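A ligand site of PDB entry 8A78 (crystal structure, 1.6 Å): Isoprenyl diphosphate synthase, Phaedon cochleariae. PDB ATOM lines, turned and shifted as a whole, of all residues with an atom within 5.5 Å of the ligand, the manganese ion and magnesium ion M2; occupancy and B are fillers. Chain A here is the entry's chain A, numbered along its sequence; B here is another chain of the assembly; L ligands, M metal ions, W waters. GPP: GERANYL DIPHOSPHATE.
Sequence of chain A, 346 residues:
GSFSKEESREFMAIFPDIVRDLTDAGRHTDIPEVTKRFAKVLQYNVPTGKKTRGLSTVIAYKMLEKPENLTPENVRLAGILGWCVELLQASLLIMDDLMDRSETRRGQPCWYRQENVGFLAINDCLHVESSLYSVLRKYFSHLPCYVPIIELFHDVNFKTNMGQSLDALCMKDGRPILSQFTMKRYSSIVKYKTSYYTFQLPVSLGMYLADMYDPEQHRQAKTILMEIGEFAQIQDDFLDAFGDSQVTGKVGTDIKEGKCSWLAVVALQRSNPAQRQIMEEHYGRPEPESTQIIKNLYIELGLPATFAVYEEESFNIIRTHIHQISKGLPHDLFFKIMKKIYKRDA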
ATOM      1  N   SER A  91      -7.924 -35.154  -6.522  1.00  0.00           N
ATOM      2  CA  SER A  91      -8.845 -34.227  -7.238  1.00  0.00           C
ATOM      3  C   SER A  91      -8.746 -32.837  -6.616  1.00  0.00           C
ATOM      4  O   SER A  91      -8.661 -31.836  -7.368  1.00  0.00           O
ATOM      5  CB  SER A  91     -10.288 -34.709  -7.223  1.00  0.00           C
ATOM      6  OG  SER A  91     -10.811 -34.642  -5.916  1.00  0.00           O
ATOM      7  N   LEU A  92      -8.759 -32.759  -5.291  1.00  0.00           N
ATOM      8  CA  LEU A  92      -8.798 -31.454  -4.589  1.00  0.00           C
ATOM      9  C   LEU A  92      -7.489 -30.704  -4.858  1.00  0.00           C
ATOM     10  O   LEU A  92      -7.560 -29.483  -5.095  1.00  0.00           O
ATOM     11  CB  LEU A  92      -9.012 -31.641  -3.092  1.00  0.00           C
ATOM     12  CG  LEU A  92     -10.343 -32.262  -2.695  1.00  0.00           C
ATOM     13  CD1 LEU A  92     -10.309 -32.585  -1.216  1.00  0.00           C
ATOM     14  CD2 LEU A  92     -11.516 -31.332  -3.014  1.00  0.00           C
ATOM     15  N   LEU A  93      -6.354 -31.405  -4.818  1.00  0.00           N
ATOM     16  CA  LEU A  93      -5.039 -30.726  -4.929  1.00  0.00           C
ATOM     17  C   LEU A  93      -4.817 -30.345  -6.398  1.00  0.00           C
ATOM     18  O   LEU A  93      -4.254 -29.270  -6.645  1.00  0.00           O
ATOM     19  CB  LEU A  93      -3.941 -31.618  -4.364  1.00  0.00           C
ATOM     20  CG  LEU A  93      -4.118 -31.995  -2.893  1.00  0.00           C
ATOM     21  CD1 LEU A  93      -2.869 -32.665  -2.343  1.00  0.00           C
ATOM     22  CD2 LEU A  93      -4.481 -30.785  -2.051  1.00  0.00           C
ATOM     23  N   MET A  95      -7.071 -29.266  -8.376  1.00  0.00           N
ATOM     24  CA  MET A  95      -7.870 -28.029  -8.538  1.00  0.00           C
ATOM     25  C   MET A  95      -7.208 -26.904  -7.744  1.00  0.00           C
ATOM     26  O   MET A  95      -7.092 -25.782  -8.296  1.00  0.00           O
ATOM     27  CB  MET A  95      -9.298 -28.215  -8.057  1.00  0.00           C
ATOM     28  CG  MET A  95     -10.128 -26.970  -8.252  1.00  0.00           C
ATOM     29  SD  MET A  95     -11.885 -27.272  -8.100  1.00  0.00           S
ATOM     30  CE  MET A  95     -12.278 -27.773  -9.773  1.00  0.00           C
ATOM     31  N   ASP A  96      -6.851 -27.148  -6.491  1.00  0.00           N
ATOM     32  CA  ASP A  96      -6.247 -26.090  -5.645  1.00  0.00           C
ATOM     33  C   ASP A  96      -4.974 -25.568  -6.308  1.00  0.00           C
ATOM     34  O   ASP A  96      -4.732 -24.345  -6.249  1.00  0.00           O
ATOM     35  CB  ASP A  96      -5.962 -26.581  -4.233  1.00  0.00           C
ATOM     36  CG  ASP A  96      -5.305 -25.509  -3.403  1.00  0.00           C
ATOM     37  OD1 ASP A  96      -6.043 -24.650  -2.869  1.00  0.00           O
ATOM     38  OD2 ASP A  96      -4.050 -25.564  -3.279  1.00  0.00           O
ATOM     39  N   ASP A  97      -4.162 -26.441  -6.886  1.00  0.00           N
ATOM     40  CA  ASP A  97      -2.878 -26.009  -7.499  1.00  0.00           C
ATOM     41  C   ASP A  97      -3.164 -25.070  -8.669  1.00  0.00           C
ATOM     42  O   ASP A  97      -2.422 -24.066  -8.825  1.00  0.00           O
ATOM     43  CB  ASP A  97      -2.007 -27.207  -7.852  1.00  0.00           C
ATOM     44  CG  ASP A  97      -1.359 -27.847  -6.631  1.00  0.00           C
ATOM     45  OD1 ASP A  97      -1.253 -27.166  -5.579  1.00  0.00           O
ATOM     46  OD2 ASP A  97      -1.002 -29.030  -6.717  1.00  0.00           O
ATOM     47  N   MET A  99      -5.938 -23.159  -8.935  1.00  0.00           N
ATOM     48  CA  MET A  99      -6.505 -21.944  -8.309  1.00  0.00           C
ATOM     49  C   MET A  99      -5.386 -21.066  -7.726  1.00  0.00           C
ATOM     50  O   MET A  99      -5.471 -19.829  -7.867  1.00  0.00           O
ATOM     51  CB  MET A  99      -7.501 -22.329  -7.204  1.00  0.00           C
ATOM     52  CG  MET A  99      -8.767 -22.940  -7.787  1.00  0.00           C
ATOM     53  SD  MET A  99      -9.992 -23.452  -6.557  1.00  0.00           S
ATOM     54  CE  MET A  99     -10.463 -21.864  -5.872  1.00  0.00           C
ATOM     55  N   ASP A 100      -4.359 -21.684  -7.148  1.00  0.00           N
ATOM     56  CA  ASP A 100      -3.266 -20.950  -6.447  1.00  0.00           C
ATOM     57  C   ASP A 100      -2.082 -20.716  -7.396  1.00  0.00           C
ATOM     58  O   ASP A 100      -1.117 -20.052  -6.951  1.00  0.00           O
ATOM     59  CB  ASP A 100      -2.851 -21.709  -5.193  1.00  0.00           C
ATOM     60  CG  ASP A 100      -3.955 -21.731  -4.148  1.00  0.00           C
ATOM     61  OD1 ASP A 100      -4.871 -20.885  -4.252  1.00  0.00           O
ATOM     62  OD2 ASP A 100      -3.864 -22.599  -3.228  1.00  0.00           O
ATOM     63  N   SER A 102       0.249 -22.687  -8.343  1.00  0.00           N
ATOM     64  CA  SER A 102       1.455 -23.199  -7.637  1.00  0.00           C
ATOM     65  C   SER A 102       2.420 -23.859  -8.634  1.00  0.00           C
ATOM     66  O   SER A 102       1.981 -24.299  -9.711  1.00  0.00           O
ATOM     67  CB  SER A 102       1.080 -24.106  -6.518  1.00  0.00           C
ATOM     68  OG  SER A 102       0.373 -23.362  -5.528  1.00  0.00           O
ATOM     69  N   ARG A 105       3.987 -29.655  -6.180  1.00  0.00           N
ATOM     70  CA  ARG A 105       3.203 -30.390  -5.157  1.00  0.00           C
ATOM     71  C   ARG A 105       3.912 -31.729  -4.983  1.00  0.00           C
ATOM     72  O   ARG A 105       4.183 -32.368  -6.014  1.00  0.00           O
ATOM     73  CB  ARG A 105       1.769 -30.487  -5.668  1.00  0.00           C
ATOM     74  CG  ARG A 105       0.893 -31.516  -4.963  1.00  0.00           C
ATOM     75  CD  ARG A 105       0.385 -31.000  -3.643  1.00  0.00           C
ATOM     76  NE  ARG A 105      -0.544 -29.896  -3.837  1.00  0.00           N
ATOM     77  CZ  ARG A 105      -0.985 -29.096  -2.871  1.00  0.00           C
ATOM     78  NH1 ARG A 105      -0.614 -29.297  -1.622  1.00  0.00           N
ATOM     79  NH2 ARG A 105      -1.815 -28.107  -3.147  1.00  0.00           N
ATOM     80  N   THR A 160     -15.916 -29.604   1.887  1.00  0.00           N
ATOM     81  CA  THR A 160     -14.540 -29.190   1.525  1.00  0.00           C
ATOM     82  C   THR A 160     -14.635 -27.983   0.569  1.00  0.00           C
ATOM     83  O   THR A 160     -13.845 -27.022   0.712  1.00  0.00           O
ATOM     84  CB  THR A 160     -13.762 -30.365   0.929  1.00  0.00           C
ATOM     85  OG1 THR A 160     -13.733 -31.441   1.876  1.00  0.00           O
ATOM     86  CG2 THR A 160     -12.355 -29.951   0.571  1.00  0.00           C
ATOM     87  N   ASN A 161     -15.594 -28.007  -0.345  1.00  0.00           N
ATOM     88  CA  ASN A 161     -15.863 -26.867  -1.261  1.00  0.00           C
ATOM     89  C   ASN A 161     -16.258 -25.643  -0.443  1.00  0.00           C
ATOM     90  O   ASN A 161     -15.788 -24.557  -0.766  1.00  0.00           O
ATOM     91  CB  ASN A 161     -16.888 -27.242  -2.318  1.00  0.00           C
ATOM     92  CG  ASN A 161     -16.220 -27.883  -3.503  1.00  0.00           C
ATOM     93  OD1 ASN A 161     -15.646 -27.148  -4.305  1.00  0.00           O
ATOM     94  ND2 ASN A 161     -16.271 -29.205  -3.608  1.00  0.00           N
ATOM     95  N   GLN A 164     -13.033 -24.253   0.873  1.00  0.00           N
ATOM     96  CA  GLN A 164     -12.181 -23.652  -0.187  1.00  0.00           C
ATOM     97  C   GLN A 164     -12.752 -22.274  -0.556  1.00  0.00           C
ATOM     98  O   GLN A 164     -11.962 -21.345  -0.730  1.00  0.00           O
ATOM     99  CB  GLN A 164     -12.161 -24.557  -1.414  1.00  0.00           C
ATOM    100  CG  GLN A 164     -11.261 -24.053  -2.549  1.00  0.00           C
ATOM    101  CD  GLN A 164      -9.782 -24.209  -2.263  1.00  0.00           C
ATOM    102  OE1 GLN A 164      -9.347 -24.235  -1.114  1.00  0.00           O
ATOM    103  NE2 GLN A 164      -8.982 -24.299  -3.322  1.00  0.00           N
ATOM    104  N   ASP A 167     -12.089 -19.815   2.292  1.00  0.00           N
ATOM    105  CA  ASP A 167     -10.662 -19.415   2.175  1.00  0.00           C
ATOM    106  C   ASP A 167     -10.560 -18.298   1.129  1.00  0.00           C
ATOM    107  O   ASP A 167      -9.897 -17.277   1.389  1.00  0.00           O
ATOM    108  CB  ASP A 167      -9.794 -20.613   1.797  1.00  0.00           C
ATOM    109  CG  ASP A 167      -8.308 -20.464   2.085  1.00  0.00           C
ATOM    110  OD1 ASP A 167      -7.928 -19.515   2.801  1.00  0.00           O
ATOM    111  OD2 ASP A 167      -7.542 -21.309   1.617  1.00  0.00           O
ATOM    112  N   LYS A 193     -12.271 -26.988   5.031  1.00  0.00           N
ATOM    113  CA  LYS A 193     -11.332 -27.190   3.904  1.00  0.00           C
ATOM    114  C   LYS A 193     -10.421 -28.399   4.119  1.00  0.00           C
ATOM    115  O   LYS A 193     -10.022 -28.980   3.122  1.00  0.00           O
ATOM    116  CB  LYS A 193     -10.461 -25.952   3.674  1.00  0.00           C
ATOM    117  CG  LYS A 193      -9.696 -25.959   2.351  1.00  0.00           C
ATOM    118  CD  LYS A 193      -8.722 -24.816   2.257  1.00  0.00           C
ATOM    119  CE  LYS A 193      -7.578 -24.868   3.239  1.00  0.00           C
ATOM    120  NZ  LYS A 193      -6.667 -23.726   3.030  1.00  0.00           N
ATOM    121  N   THR A 194     -10.087 -28.774   5.349  1.00  0.00           N
ATOM    122  CA  THR A 194      -8.993 -29.736   5.573  1.00  0.00           C
ATOM    123  C   THR A 194      -9.398 -30.846   6.548  1.00  0.00           C
ATOM    124  O   THR A 194      -9.162 -32.035   6.211  1.00  0.00           O
ATOM    125  CB  THR A 194      -7.702 -29.049   6.010  1.00  0.00           C
ATOM    126  OG1 THR A 194      -7.426 -28.007   5.068  1.00  0.00           O
ATOM    127  CG2 THR A 194      -6.563 -30.031   6.034  1.00  0.00           C
ATOM    128  N   TYR A 197     -11.945 -33.919   5.405  1.00  0.00           N
ATOM    129  CA  TYR A 197     -11.450 -34.966   4.478  1.00  0.00           C
ATOM    130  C   TYR A 197     -10.199 -35.630   5.060  1.00  0.00           C
ATOM    131  O   TYR A 197      -9.938 -36.797   4.736  1.00  0.00           O
ATOM    132  CB  TYR A 197     -11.249 -34.434   3.050  1.00  0.00           C
ATOM    133  CG  TYR A 197      -9.867 -33.950   2.702  1.00  0.00           C
ATOM    134  CD1 TYR A 197      -8.904 -34.812   2.180  1.00  0.00           C
ATOM    135  CD2 TYR A 197      -9.530 -32.616   2.851  1.00  0.00           C
ATOM    136  CE1 TYR A 197      -7.641 -34.355   1.837  1.00  0.00           C
ATOM    137  CE2 TYR A 197      -8.273 -32.142   2.509  1.00  0.00           C
ATOM    138  CZ  TYR A 197      -7.319 -33.027   2.026  1.00  0.00           C
ATOM    139  OH  TYR A 197      -6.067 -32.598   1.691  1.00  0.00           O
ATOM    140  N   ASP A 254       3.631 -19.166   2.273  1.00  0.00           N
ATOM    141  CA  ASP A 254       2.297 -18.738   2.785  1.00  0.00           C
ATOM    142  C   ASP A 254       2.227 -17.206   2.822  1.00  0.00           C
ATOM    143  O   ASP A 254       1.163 -16.659   2.470  1.00  0.00           O
ATOM    144  CB  ASP A 254       1.999 -19.292   4.183  1.00  0.00           C
ATOM    145  CG  ASP A 254       1.706 -20.778   4.236  1.00  0.00           C
ATOM    146  OD1 ASP A 254       1.627 -21.399   3.158  1.00  0.00           O
ATOM    147  OD2 ASP A 254       1.549 -21.289   5.364  1.00  0.00           O
ATOM    148  N   GLU A 257       1.845 -15.699  -0.616  1.00  0.00           N
ATOM    149  CA  GLU A 257       0.521 -16.092  -1.183  1.00  0.00           C
ATOM    150  C   GLU A 257      -0.612 -15.344  -0.468  1.00  0.00           C
ATOM    151  O   GLU A 257      -1.756 -15.426  -0.948  1.00  0.00           O
ATOM    152  CB  GLU A 257       0.305 -17.608  -1.053  1.00  0.00           C
ATOM    153  CG  GLU A 257       1.133 -18.405  -2.031  1.00  0.00           C
ATOM    154  CD  GLU A 257       0.847 -19.906  -2.016  1.00  0.00           C
ATOM    155  OE1 GLU A 257      -0.282 -20.324  -2.425  1.00  0.00           O
ATOM    156  OE2 GLU A 257       1.748 -20.657  -1.590  1.00  0.00           O
ATOM    157  N   LYS A 259      -1.836 -16.060   2.570  1.00  0.00           N
ATOM    158  CA  LYS A 259      -2.723 -17.113   3.145  1.00  0.00           C
ATOM    159  C   LYS A 259      -3.278 -16.627   4.481  1.00  0.00           C
ATOM    160  O   LYS A 259      -2.552 -15.920   5.213  1.00  0.00           O
ATOM    161  CB  LYS A 259      -1.977 -18.433   3.358  1.00  0.00           C
ATOM    162  CG  LYS A 259      -1.846 -19.265   2.092  1.00  0.00           C
ATOM    163  CD  LYS A 259      -1.550 -20.694   2.383  1.00  0.00           C
ATOM    164  CE  LYS A 259      -1.116 -21.463   1.153  1.00  0.00           C
ATOM    165  NZ  LYS A 259      -0.488 -22.740   1.544  1.00  0.00           N
ATOM    166  N   ASN B 123     -13.701 -23.612  -8.181  1.00  0.00           N
ATOM    167  CA  ASN B 123     -14.267 -24.791  -7.466  1.00  0.00           C
ATOM    168  C   ASN B 123     -15.803 -24.747  -7.465  1.00  0.00           C
ATOM    169  O   ASN B 123     -16.414 -25.759  -7.072  1.00  0.00           O
ATOM    170  CB  ASN B 123     -13.722 -24.940  -6.054  1.00  0.00           C
ATOM    171  CG  ASN B 123     -14.125 -23.815  -5.133  1.00  0.00           C
ATOM    172  OD1 ASN B 123     -13.766 -22.668  -5.388  1.00  0.00           O
ATOM    173  ND2 ASN B 123     -14.859 -24.138  -4.068  1.00  0.00           N
ATOM    174  N   LEU B 126     -17.227 -27.859  -9.282  1.00  0.00           N
ATOM    175  CA  LEU B 126     -17.183 -29.069  -8.413  1.00  0.00           C
ATOM    176  C   LEU B 126     -18.280 -28.984  -7.355  1.00  0.00           C
ATOM    177  O   LEU B 126     -18.979 -30.000  -7.102  1.00  0.00           O
ATOM    178  CB  LEU B 126     -15.799 -29.125  -7.755  1.00  0.00           C
ATOM    179  CG  LEU B 126     -15.547 -30.320  -6.839  1.00  0.00           C
ATOM    180  CD1 LEU B 126     -15.691 -31.611  -7.605  1.00  0.00           C
ATOM    181  CD2 LEU B 126     -14.171 -30.231  -6.183  1.00  0.00           C
HETATM  182  C1  GPP L   1      -4.944 -26.735  -0.108  1.00  0.00           C
HETATM  183  O1  GPP L   1      -4.927 -25.625   0.779  1.00  0.00           O
HETATM  184  C2  GPP L   1      -6.376 -27.066  -0.437  1.00  0.00           C
HETATM  185  C3  GPP L   1      -7.080 -28.108   0.015  1.00  0.00           C
HETATM  186  C4  GPP L   1      -6.560 -29.078   1.035  1.00  0.00           C
HETATM  187  C5  GPP L   1      -8.494 -28.391  -0.429  1.00  0.00           C
HETATM  188  C6  GPP L   1      -8.934 -27.684  -1.724  1.00  0.00           C
HETATM  189  C7  GPP L   1     -10.402 -27.755  -1.953  1.00  0.00           C
HETATM  190  C8  GPP L   1     -11.066 -27.685  -3.094  1.00  0.00           C
HETATM  191  C9  GPP L   1     -10.408 -27.589  -4.462  1.00  0.00           C
HETATM  192  C10 GPP L   1     -12.566 -27.645  -3.111  1.00  0.00           C
HETATM  193  PA  GPP L   1      -3.925 -24.400   0.571  1.00  0.00           P
HETATM  194  O1A GPP L   1      -3.890 -23.912  -0.856  1.00  0.00           O
HETATM  195  O2A GPP L   1      -4.166 -23.438   1.690  1.00  0.00           O
HETATM  196  O3A GPP L   1      -2.522 -25.098   0.913  1.00  0.00           O
HETATM  197  PB  GPP L   1      -1.362 -25.668  -0.028  1.00  0.00           P
HETATM  198  O1B GPP L   1      -1.785 -25.553  -1.478  1.00  0.00           O
HETATM  199  O2B GPP L   1      -1.232 -27.115   0.428  1.00  0.00           O
HETATM  200  O3B GPP L   1      -0.172 -24.830   0.322  1.00  0.00           O
HETATM  201 MN    MN M   1      -5.557 -22.863  -1.896  1.00  0.00          MN
HETATM  202 MG    MG M   2      -2.683 -24.173  -2.558  1.00  0.00          MG
HETATM  203 MG    MG M   3       0.930 -25.376   4.768  1.00  0.00          MG
HETATM  204  O   HOH W   1      -7.090 -21.815  -3.056  1.00  0.00           O
HETATM  205  O   HOH W   2      -4.955 -30.752   3.242  1.00  0.00           O
HETATM  206  O   HOH W   3       2.009 -25.080  -0.844  1.00  0.00           O
HETATM  207  O   HOH W   4      -1.238 -22.702  -2.077  1.00  0.00           O
HETATM  208  O   HOH W   5       1.316 -24.267   3.078  1.00  0.00           O
HETATM  209  O   HOH W   6      -1.610 -24.682  -4.251  1.00  0.00           O
HETATM  210  O   HOH W   7      -5.050 -20.978  -1.036  1.00  0.00           O
HETATM  211  O   HOH W   8      -2.374 -23.442   3.805  1.00  0.00           O
HETATM  212  O   HOH W   9      -4.950 -21.002   1.591  1.00  0.00           O
HETATM  213  O   HOH W  10      -2.500 -27.760   2.723  1.00  0.00           O
HETATM  214  O   HOH W  11      -7.022 -23.198  -0.350  1.00  0.00           O
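An oxygen (O2B) of the ligand lies within salt-bridge range of the guanidinium group (NH1) of Arg 105 (3.1 Å).
NZ of Lys 193 lies within salt-bridge range of O2A of the ligand, at 2.9 Å.
NZ of Lys 259 is in salt-bridge range of O3B of the ligand (2.4 Å).
OD1 of Asp 254 lies within salt-bridge range of NZ of Lys 259, 3.0 Å away.
The side-chain carboxylate (OD1) of Asp 97 is in salt-bridge range of the guanidinium group (NH2) of Arg 105, at 2.7 Å.
The side-chain carboxylate (OD2) of Asp 167 lies within salt-bridge range of the side-chain amino group (NZ) of Lys 193.
SD of Met 99 sits at hydrogen-bond distance from NE2 of Gln 164.
OD2 of Asp 96 sits close to NH2 of Arg 105 (3.4 Å).
The side-chain carboxylate (OD1) of Asp 96 sits close to the side-chain amide nitrogen (NE2) of Gln 164 (3.0 Å).
OD1 of Asn 161 is in hydrogen-bond range of ND2 of Asn 123 of chain B (3.1 Å).
Leu 92 touches the ligand.
CB of Met 95 touches C9 of the ligand, 3.8 Å away.
Thr 160 touches the ligand (CG2 to C7, 3.9 Å).
Asn 161 touches the ligand (OD1 to C10, 3.3 Å).
Gln 164 touches the ligand (OE1 to C6, 3.5 Å).
Asp 167 touches the ligand (OD2 to O2A, 3.99 Å).
Tyr 197 touches the ligand (OH to C4, 3.6 Å).
Hydrophobic or aromatic side chains that line the ligand: Leu 92, Met 95 and Tyr 197.
Gln 164 touches the manganese ion (NE2 to MN, 3.98 Å).
The nearest printed residue that does not touch the manganese ion is Asp 167 (4.3 Å).
Of the 22 residues printed, 2 come within 4 Å of magnesium ion M2.
Along chain A the residues within 4 Å of magnesium ion M2 span positions 96 to 100.
The nearest printed residue that does not touch magnesium ion M2 is Arg 105 (4.1 Å).
The manganese ion is bound by the side-chain carboxylate (OD1) of Asp 96 (2.1 Å), water W7 (2.1 Å), water W11 (2.2 Å), the side-chain carboxylate (OD2) of Asp 100 (2.2 Å), water W1 (2.2 Å) and an oxygen (O1A) of the ligand (2.2 Å).
The manganese ion has six donor atoms within binding distance.
Magnesium ion M2 is bound by an oxygen (O1B) of the ligand (2.0 Å), water W6 (2.1 Å), the side-chain carboxylate of Asp 100 (2.1 Å), the side-chain carboxylate of Asp 96 (2.1 Å), an oxygen (O1A) of the ligand (2.1 Å) and water W4 (2.1 Å).
Water W1 lies within hydrogen-bond range of OD1 of Asp 100 and NE2 of Gln 164.
Water W6 bridges OG of Ser 102 (2.7 Å) and OD1 of Asp 97 (2.8 Å).
Water W4 lies within hydrogen-bond range of OE1 of Glu 257 (2.6 Å) and O3B of the ligand (3.4 Å).
Water W9 bridges O2A of the ligand (2.6 Å) and OD2 of Asp 167 (2.6 Å).
Water W8 bridges O2A of the ligand (2.8 Å) and NZ of Lys 259 (3.0 Å).
Water W5 lies within hydrogen-bond range of the side-chain amino group of Lys 259 (2.8 Å), the side-chain carboxylate of Asp 254 (2.9 Å) and an oxygen (O3B) of the ligand (3.2 Å).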
